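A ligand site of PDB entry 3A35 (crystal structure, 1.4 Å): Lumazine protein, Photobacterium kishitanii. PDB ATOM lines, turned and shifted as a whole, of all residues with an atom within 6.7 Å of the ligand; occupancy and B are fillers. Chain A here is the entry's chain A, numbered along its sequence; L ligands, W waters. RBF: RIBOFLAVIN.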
ATOM      1  N   VAL A  41      11.651  28.023 -21.998  1.00  0.00           N
ATOM      2  CA  VAL A  41      11.980  27.396 -23.266  1.00  0.00           C
ATOM      3  C   VAL A  41      12.066  28.576 -24.224  1.00  0.00           C
ATOM      4  O   VAL A  41      11.129  29.325 -24.454  1.00  0.00           O
ATOM      5  CB  VAL A  41      10.892  26.405 -23.725  1.00  0.00           C
ATOM      6  CG1 VAL A  41      11.272  25.902 -25.116  1.00  0.00           C
ATOM      7  CG2 VAL A  41      10.918  25.232 -22.793  1.00  0.00           C
ATOM      8  N   GLY A  46      18.168  29.971 -32.819  1.00  0.00           N
ATOM      9  CA  GLY A  46      16.993  29.416 -33.516  1.00  0.00           C
ATOM     10  C   GLY A  46      16.574  28.082 -32.993  1.00  0.00           C
ATOM     11  O   GLY A  46      15.499  27.546 -33.456  1.00  0.00           O
ATOM     12  N   CYS A  47      17.250  27.504 -31.983  1.00  0.00           N
ATOM     13  CA  CYS A  47      16.864  26.170 -31.493  1.00  0.00           C
ATOM     14  C   CYS A  47      16.134  26.318 -30.146  1.00  0.00           C
ATOM     15  O   CYS A  47      16.641  26.944 -29.238  1.00  0.00           O
ATOM     16  CB  CYS A  47      18.151  25.427 -31.236  1.00  0.00           C
ATOM     17  SG  CYS A  47      17.918  23.682 -30.721  1.00  0.00           S
ATOM     18  N   SER A  48      14.982  25.629 -30.030  1.00  0.00           N
ATOM     19  CA  SER A  48      14.312  25.606 -28.755  1.00  0.00           C
ATOM     20  C   SER A  48      15.196  24.816 -27.732  1.00  0.00           C
ATOM     21  O   SER A  48      15.450  23.630 -27.929  1.00  0.00           O
ATOM     22  CB  SER A  48      12.942  24.953 -28.835  1.00  0.00           C
ATOM     23  OG  SER A  48      12.009  25.831 -29.474  1.00  0.00           O
ATOM     24  N   LEU A  49      15.481  25.466 -26.611  1.00  0.00           N
ATOM     25  CA  LEU A  49      16.227  24.887 -25.462  1.00  0.00           C
ATOM     26  C   LEU A  49      15.577  25.351 -24.184  1.00  0.00           C
ATOM     27  O   LEU A  49      14.960  26.418 -24.104  1.00  0.00           O
ATOM     28  CB  LEU A  49      17.723  25.294 -25.449  1.00  0.00           C
ATOM     29  CG  LEU A  49      18.523  24.922 -26.692  1.00  0.00           C
ATOM     30  CD1 LEU A  49      19.956  25.488 -26.567  1.00  0.00           C
ATOM     31  CD2 LEU A  49      18.606  23.371 -26.896  1.00  0.00           C
ATOM     32  N   THR A  50      15.777  24.552 -23.158  1.00  0.00           N
ATOM     33  CA  THR A  50      15.179  24.815 -21.820  1.00  0.00           C
ATOM     34  C   THR A  50      16.234  25.304 -20.831  1.00  0.00           C
ATOM     35  O   THR A  50      17.251  24.632 -20.658  1.00  0.00           O
ATOM     36  CB  THR A  50      14.574  23.448 -21.323  1.00  0.00           C
ATOM     37  OG1 THR A  50      13.649  22.979 -22.318  1.00  0.00           O
ATOM     38  CG2 THR A  50      13.838  23.764 -19.948  1.00  0.00           C
ATOM     39  N   VAL A  51      15.946  26.390 -20.140  1.00  0.00           N
ATOM     40  CA  VAL A  51      16.955  26.813 -19.145  1.00  0.00           C
ATOM     41  C   VAL A  51      17.029  25.816 -17.983  1.00  0.00           C
ATOM     42  O   VAL A  51      15.947  25.510 -17.404  1.00  0.00           O
ATOM     43  CB  VAL A  51      16.567  28.215 -18.646  1.00  0.00           C
ATOM     44  CG1 VAL A  51      17.461  28.660 -17.493  1.00  0.00           C
ATOM     45  CG2 VAL A  51      16.545  29.272 -19.759  1.00  0.00           C
ATOM     46  N   VAL A  52      18.241  25.413 -17.649  1.00  0.00           N
ATOM     47  CA  VAL A  52      18.427  24.452 -16.544  1.00  0.00           C
ATOM     48  C   VAL A  52      18.832  25.208 -15.277  1.00  0.00           C
ATOM     49  O   VAL A  52      18.533  24.674 -14.199  1.00  0.00           O
ATOM     50  CB  VAL A  52      19.577  23.511 -16.969  1.00  0.00           C
ATOM     51  CG1 VAL A  52      20.315  22.922 -15.722  1.00  0.00           C
ATOM     52  CG2 VAL A  52      19.051  22.517 -18.008  1.00  0.00           C
ATOM     53  N   PHE A  61      22.107  25.732 -20.328  1.00  0.00           N
ATOM     54  CA  PHE A  61      21.261  24.837 -21.126  1.00  0.00           C
ATOM     55  C   PHE A  61      21.964  23.544 -21.297  1.00  0.00           C
ATOM     56  O   PHE A  61      23.175  23.493 -21.522  1.00  0.00           O
ATOM     57  CB  PHE A  61      21.023  25.440 -22.589  1.00  0.00           C
ATOM     58  CG  PHE A  61      20.370  26.790 -22.590  1.00  0.00           C
ATOM     59  CD1 PHE A  61      18.958  26.870 -22.644  1.00  0.00           C
ATOM     60  CD2 PHE A  61      21.118  27.930 -22.532  1.00  0.00           C
ATOM     61  CE1 PHE A  61      18.325  28.078 -22.634  1.00  0.00           C
ATOM     62  CE2 PHE A  61      20.438  29.224 -22.520  1.00  0.00           C
ATOM     63  CZ  PHE A  61      19.080  29.268 -22.581  1.00  0.00           C
ATOM     64  N   ASP A  62      21.218  22.438 -21.290  1.00  0.00           N
ATOM     65  CA  ASP A  62      21.757  21.161 -21.793  1.00  0.00           C
ATOM     66  C   ASP A  62      21.389  20.866 -23.232  1.00  0.00           C
ATOM     67  O   ASP A  62      20.117  20.998 -23.551  1.00  0.00           O
ATOM     68  CB  ASP A  62      21.214  20.051 -20.857  1.00  0.00           C
ATOM     69  CG  ASP A  62      21.862  19.999 -19.537  1.00  0.00           C
ATOM     70  OD1 ASP A  62      23.091  20.271 -19.450  1.00  0.00           O
ATOM     71  OD2 ASP A  62      21.261  19.602 -18.484  1.00  0.00           O
ATOM     72  N   ILE A  63      22.340  20.548 -24.046  1.00  0.00           N
ATOM     73  CA  ILE A  63      22.069  20.231 -25.425  1.00  0.00           C
ATOM     74  C   ILE A  63      22.236  18.710 -25.459  1.00  0.00           C
ATOM     75  O   ILE A  63      23.321  18.178 -25.273  1.00  0.00           O
ATOM     76  CB  ILE A  63      23.077  20.949 -26.359  1.00  0.00           C
ATOM     77  CG1 ILE A  63      22.884  22.528 -26.189  1.00  0.00           C
ATOM     78  CG2 ILE A  63      22.793  20.649 -27.833  1.00  0.00           C
ATOM     79  CD1 ILE A  63      23.856  23.148 -25.429  1.00  0.00           C
ATOM     80  N   ASP A  64      21.130  18.043 -25.779  1.00  0.00           N
ATOM     81  CA  ASP A  64      21.080  16.542 -25.776  1.00  0.00           C
ATOM     82  C   ASP A  64      20.270  16.134 -26.996  1.00  0.00           C
ATOM     83  O   ASP A  64      20.802  15.695 -27.977  1.00  0.00           O
ATOM     84  CB  ASP A  64      20.587  16.023 -24.443  1.00  0.00           C
ATOM     85  CG  ASP A  64      19.456  16.765 -23.807  1.00  0.00           C
ATOM     86  OD1 ASP A  64      18.505  17.317 -24.404  1.00  0.00           O
ATOM     87  OD2 ASP A  64      19.368  16.774 -22.538  1.00  0.00           O
ATOM     88  N   GLN A  65      18.922  16.368 -26.879  1.00  0.00           N
ATOM     89  CA  GLN A  65      18.109  16.042 -28.019  1.00  0.00           C
ATOM     90  C   GLN A  65      18.526  16.704 -29.296  1.00  0.00           C
ATOM     91  O   GLN A  65      18.437  16.218 -30.396  1.00  0.00           O
ATOM     92  CB  GLN A  65      16.717  16.420 -27.637  1.00  0.00           C
ATOM     93  CG  GLN A  65      15.677  16.066 -28.698  1.00  0.00           C
ATOM     94  CD  GLN A  65      14.264  16.496 -28.229  1.00  0.00           C
ATOM     95  OE1 GLN A  65      13.956  16.707 -27.059  1.00  0.00           O
ATOM     96  NE2 GLN A  65      13.423  16.629 -29.245  1.00  0.00           N
ATOM     97  N   ALA A  66      19.043  17.981 -29.145  1.00  0.00           N
ATOM     98  CA  ALA A  66      19.421  18.737 -30.289  1.00  0.00           C
ATOM     99  C   ALA A  66      20.847  18.561 -30.796  1.00  0.00           C
ATOM    100  O   ALA A  66      21.248  19.137 -31.800  1.00  0.00           O
ATOM    101  CB  ALA A  66      19.286  20.257 -29.920  1.00  0.00           C
ATOM    102  N   ILE A  67      21.582  17.633 -30.135  1.00  0.00           N
ATOM    103  CA  ILE A  67      23.087  17.651 -30.333  1.00  0.00           C
ATOM    104  C   ILE A  67      23.524  17.207 -31.734  1.00  0.00           C
ATOM    105  O   ILE A  67      24.622  17.567 -32.201  1.00  0.00           O
ATOM    106  CB  ILE A  67      23.739  16.830 -29.267  1.00  0.00           C
ATOM    107  CG1 ILE A  67      25.222  17.214 -29.199  1.00  0.00           C
ATOM    108  CG2 ILE A  67      23.657  15.348 -29.611  1.00  0.00           C
ATOM    109  CD1 ILE A  67      25.871  16.847 -27.955  1.00  0.00           C
ATOM    110  N   ASN A  68      22.710  16.412 -32.416  1.00  0.00           N
ATOM    111  CA  ASN A  68      23.078  15.850 -33.727  1.00  0.00           C
ATOM    112  C   ASN A  68      22.620  16.630 -34.900  1.00  0.00           C
ATOM    113  O   ASN A  68      22.929  16.285 -36.077  1.00  0.00           O
ATOM    114  CB  ASN A  68      22.490  14.417 -33.843  1.00  0.00           C
ATOM    115  CG  ASN A  68      23.092  13.499 -32.823  1.00  0.00           C
ATOM    116  OD1 ASN A  68      22.402  12.875 -32.043  1.00  0.00           O
ATOM    117  ND2 ASN A  68      24.416  13.447 -32.837  1.00  0.00           N
ATOM    118  N   THR A  69      21.768  17.709 -34.672  1.00  0.00           N
ATOM    119  CA  THR A  69      21.184  18.433 -35.837  1.00  0.00           C
ATOM    120  C   THR A  69      21.361  19.961 -35.716  1.00  0.00           C
ATOM    121  O   THR A  69      20.746  20.713 -36.428  1.00  0.00           O
ATOM    122  CB  THR A  69      19.644  18.157 -35.823  1.00  0.00           C
ATOM    123  OG1 THR A  69      19.138  18.321 -34.515  1.00  0.00           O
ATOM    124  CG2 THR A  69      19.399  16.699 -36.286  1.00  0.00           C
ATOM    125  N   THR A  70      22.336  20.348 -34.870  1.00  0.00           N
ATOM    126  CA  THR A  70      22.632  21.795 -34.642  1.00  0.00           C
ATOM    127  C   THR A  70      24.123  22.024 -34.523  1.00  0.00           C
ATOM    128  O   THR A  70      24.909  21.058 -34.435  1.00  0.00           O
ATOM    129  CB  THR A  70      21.944  22.302 -33.306  1.00  0.00           C
ATOM    130  OG1 THR A  70      22.500  21.517 -32.224  1.00  0.00           O
ATOM    131  CG2 THR A  70      20.414  22.092 -33.346  1.00  0.00           C
ATOM    132  N   ARG A  86      10.016  33.943 -26.096  1.00  0.00           N
ATOM    133  CA  ARG A  86       8.693  33.911 -26.730  1.00  0.00           C
ATOM    134  C   ARG A  86       7.924  35.209 -26.501  1.00  0.00           C
ATOM    135  O   ARG A  86       8.086  35.820 -25.441  1.00  0.00           O
ATOM    136  CB  ARG A  86       7.827  32.742 -26.314  1.00  0.00           C
ATOM    137  CG  ARG A  86       7.374  32.693 -24.964  1.00  0.00           C
ATOM    138  CD  ARG A  86       6.398  31.477 -24.879  1.00  0.00           C
ATOM    139  NE  ARG A  86       7.345  30.360 -24.755  1.00  0.00           N
ATOM    140  CZ  ARG A  86       7.539  29.431 -25.683  1.00  0.00           C
ATOM    141  NH1 ARG A  86       6.885  29.501 -26.832  1.00  0.00           N
ATOM    142  NH2 ARG A  86       8.443  28.514 -25.493  1.00  0.00           N
ATOM    143  N   THR A  99       9.356  27.710 -35.267  1.00  0.00           N
ATOM    144  CA  THR A  99       9.030  26.779 -34.210  1.00  0.00           C
ATOM    145  C   THR A  99      10.153  26.434 -33.224  1.00  0.00           C
ATOM    146  O   THR A  99       9.892  26.013 -32.114  1.00  0.00           O
ATOM    147  CB  THR A  99       8.574  25.397 -34.753  1.00  0.00           C
ATOM    148  OG1 THR A  99       9.632  24.693 -35.392  1.00  0.00           O
ATOM    149  CG2 THR A  99       7.390  25.474 -35.711  1.00  0.00           C
ATOM    150  N   GLY A 100      11.397  26.722 -33.692  1.00  0.00           N
ATOM    151  CA  GLY A 100      12.555  26.299 -32.806  1.00  0.00           C
ATOM    152  C   GLY A 100      13.029  24.891 -33.132  1.00  0.00           C
ATOM    153  O   GLY A 100      13.949  24.396 -32.458  1.00  0.00           O
ATOM    154  N   ASN A 101      12.451  24.174 -34.060  1.00  0.00           N
ATOM    155  CA  ASN A 101      12.868  22.791 -34.443  1.00  0.00           C
ATOM    156  C   ASN A 101      13.826  22.977 -35.592  1.00  0.00           C
ATOM    157  O   ASN A 101      13.431  23.222 -36.746  1.00  0.00           O
ATOM    158  CB  ASN A 101      11.672  21.933 -34.957  1.00  0.00           C
ATOM    159  CG  ASN A 101      12.152  20.558 -35.380  1.00  0.00           C
ATOM    160  OD1 ASN A 101      11.928  20.146 -36.500  1.00  0.00           O
ATOM    161  ND2 ASN A 101      12.770  19.880 -34.534  1.00  0.00           N
ATOM    162  N   ILE A 102      15.164  22.961 -35.320  1.00  0.00           N
ATOM    163  CA  ILE A 102      16.099  23.100 -36.392  1.00  0.00           C
ATOM    164  C   ILE A 102      16.147  21.786 -37.246  1.00  0.00           C
ATOM    165  O   ILE A 102      16.251  20.703 -36.720  1.00  0.00           O
ATOM    166  CB  ILE A 102      17.524  23.365 -35.759  1.00  0.00           C
ATOM    167  CG1 ILE A 102      17.538  24.724 -34.970  1.00  0.00           C
ATOM    168  CG2 ILE A 102      18.625  23.230 -36.740  1.00  0.00           C
ATOM    169  CD1 ILE A 102      17.150  25.865 -35.888  1.00  0.00           C
ATOM    170  N   LYS A 103      16.085  22.006 -38.505  1.00  0.00           N
ATOM    171  CA  LYS A 103      16.110  20.867 -39.490  1.00  0.00           C
ATOM    172  C   LYS A 103      17.476  20.328 -39.655  1.00  0.00           C
ATOM    173  O   LYS A 103      17.603  19.101 -39.972  1.00  0.00           O
ATOM    174  CB  LYS A 103      15.546  21.348 -40.793  1.00  0.00           C
ATOM    175  CG  LYS A 103      14.133  21.829 -40.617  1.00  0.00           C
ATOM    176  CD  LYS A 103      13.259  20.957 -39.686  1.00  0.00           C
ATOM    177  CE  LYS A 103      11.805  21.461 -39.764  1.00  0.00           C
ATOM    178  NZ  LYS A 103      11.032  21.129 -38.519  1.00  0.00           N
ATOM    179  N   GLY A 104      18.524  21.119 -39.588  1.00  0.00           N
ATOM    180  CA  GLY A 104      19.863  20.540 -39.627  1.00  0.00           C
ATOM    181  C   GLY A 104      20.845  21.686 -39.833  1.00  0.00           C
ATOM    182  O   GLY A 104      20.495  22.887 -39.828  1.00  0.00           O
ATOM    183  N   VAL A 180      19.648  25.684 -39.527  1.00  0.00           N
ATOM    184  CA  VAL A 180      18.541  26.071 -40.501  1.00  0.00           C
ATOM    185  C   VAL A 180      17.227  25.521 -40.036  1.00  0.00           C
ATOM    186  O   VAL A 180      17.129  24.309 -39.615  1.00  0.00           O
ATOM    187  CB  VAL A 180      18.939  25.479 -41.897  1.00  0.00           C
ATOM    188  CG1 VAL A 180      17.774  25.759 -42.922  1.00  0.00           C
ATOM    189  CG2 VAL A 180      20.292  25.920 -42.365  1.00  0.00           C
HETATM  190  N1  RBF L   1      16.765  20.026 -27.151  1.00  0.00           N
HETATM  191  C2  RBF L   1      17.855  20.020 -26.341  1.00  0.00           C
HETATM  192  O2  RBF L   1      18.946  19.499 -26.724  1.00  0.00           O
HETATM  193  N3  RBF L   1      17.871  20.623 -25.096  1.00  0.00           N
HETATM  194  C4  RBF L   1      16.737  21.305 -24.599  1.00  0.00           C
HETATM  195  O4  RBF L   1      16.812  21.830 -23.488  1.00  0.00           O
HETATM  196  C4A RBF L   1      15.595  21.223 -25.427  1.00  0.00           C
HETATM  197  N5  RBF L   1      14.377  21.797 -24.903  1.00  0.00           N
HETATM  198  C5A RBF L   1      13.264  21.731 -25.733  1.00  0.00           C
HETATM  199  C6  RBF L   1      12.063  22.175 -25.178  1.00  0.00           C
HETATM  200  C7  RBF L   1      10.925  22.066 -26.021  1.00  0.00           C
HETATM  201  C7M RBF L   1       9.586  22.507 -25.371  1.00  0.00           C
HETATM  202  C8  RBF L   1      10.971  21.596 -27.303  1.00  0.00           C
HETATM  203  C8M RBF L   1       9.752  21.587 -28.116  1.00  0.00           C
HETATM  204  C9  RBF L   1      12.222  21.166 -27.871  1.00  0.00           C
HETATM  205  C9A RBF L   1      13.341  21.152 -27.040  1.00  0.00           C
HETATM  206  N10 RBF L   1      14.593  20.628 -27.523  1.00  0.00           N
HETATM  207  C10 RBF L   1      15.658  20.621 -26.657  1.00  0.00           C
HETATM  208  C1' RBF L   1      14.711  19.963 -28.752  1.00  0.00           C
HETATM  209  C2' RBF L   1      15.385  20.747 -29.857  1.00  0.00           C
HETATM  210  O2' RBF L   1      14.683  22.022 -30.042  1.00  0.00           O
HETATM  211  C3' RBF L   1      15.337  20.038 -31.107  1.00  0.00           C
HETATM  212  O3' RBF L   1      16.044  18.713 -30.812  1.00  0.00           O
HETATM  213  C4' RBF L   1      16.216  20.650 -32.210  1.00  0.00           C
HETATM  214  O4' RBF L   1      15.596  21.853 -32.698  1.00  0.00           O
HETATM  215  C5' RBF L   1      16.395  19.702 -33.414  1.00  0.00           C
HETATM  216  O5' RBF L   1      17.321  20.217 -34.375  1.00  0.00           O
HETATM  217  O   HOH W   1      18.361  22.292 -21.298  1.00  0.00           O
HETATM  218  O   HOH W   2      10.145  23.633 -30.919  1.00  0.00           O
HETATM  219  O   HOH W   3      12.107  21.728 -31.335  1.00  0.00           O
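N of Asp 64 lies within hydrogen-bond range of O2 of the ligand (2.8 Å).
N of Ala 66 sits at hydrogen-bond distance from O2 of the ligand.
N3 of the ligand lies close to OD1 of Asp 64, 3.4 Å away.
An oxygen (O4') of the ligand lies within hydrogen-bond range of the backbone NH of Ile 102.
O of Ile 102 lies within hydrogen-bond range of O5' of the ligand (2.6 Å).
The side-chain sulfur of Cys 47 is in hydrogen-bond range of an oxygen (O4') of the ligand (3.6 Å).
N5 of the ligand sits at hydrogen-bond distance from OG1 of Thr 50 (2.9 Å).
O of Ser 48 lies within hydrogen-bond range of O2' of the ligand (2.8 Å).
The backbone carbonyl oxygen (O) of Asp 62 sits at hydrogen-bond distance from a nitrogen (N3) of the ligand, at 2.8 Å.
The backbone carbonyl oxygen (O) of Gly 100 lies within hydrogen-bond range of an oxygen (O4') of the ligand (3.0 Å).
O of Gln 65 sits close to O3' of the ligand, 3.5 Å away.
An oxygen (O2) of the ligand is in hydrogen-bond range of the backbone NH (N) of Gln 65.
OG1 of Thr 69 lies within hydrogen-bond range of O5' of the ligand (2.6 Å).
An oxygen (O4) of the ligand is in hydrogen-bond range of the backbone NH (N) of Thr 50.
O of Val 41 sits at hydrogen-bond distance from NH2 of Arg 86.
The backbone carbonyl oxygen of Ala 66 lies within hydrogen-bond range of the side-chain hydroxyl of Thr 70, 2.7 Å away.
OD1 of Asn 101 is in hydrogen-bond range of NZ of Lys 103 (2.4 Å).
The backbone NH (N) of Asn 101 lies within hydrogen-bond range of the side-chain hydroxyl (OG1) of Thr 99.
O of Thr 99 is in hydrogen-bond range of OG of Ser 48 (3.4 Å).
The backbone NH (N) of Ser 48 sits at hydrogen-bond distance from the backbone carbonyl oxygen (O) of Gly 100 (2.9 Å).
Val 41 touches the ligand (CG1 to C7M, 3.8 Å).
Leu 49 touches the ligand.
CA of Ile 63 touches O2 of the ligand, 3.5 Å away.
CG2 of Thr 70 touches O5' of the ligand, 3.8 Å away.
CA of Asn 101 touches O4' of the ligand (3.4 Å).
Water W1 lies within hydrogen-bond range of O of Thr 50 (2.7 Å), O4 of the ligand (2.7 Å) and N of Asp 62 (2.9 Å).
Water W3 lies within hydrogen-bond range of O2' of the ligand (2.9 Å) and O of Gly 100 (3.4 Å).
Water W2 bridges the backbone carbonyl oxygen (O) of Thr 99 (2.7 Å) and the side-chain hydroxyl (OG) of Ser 48 (3.2 Å).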
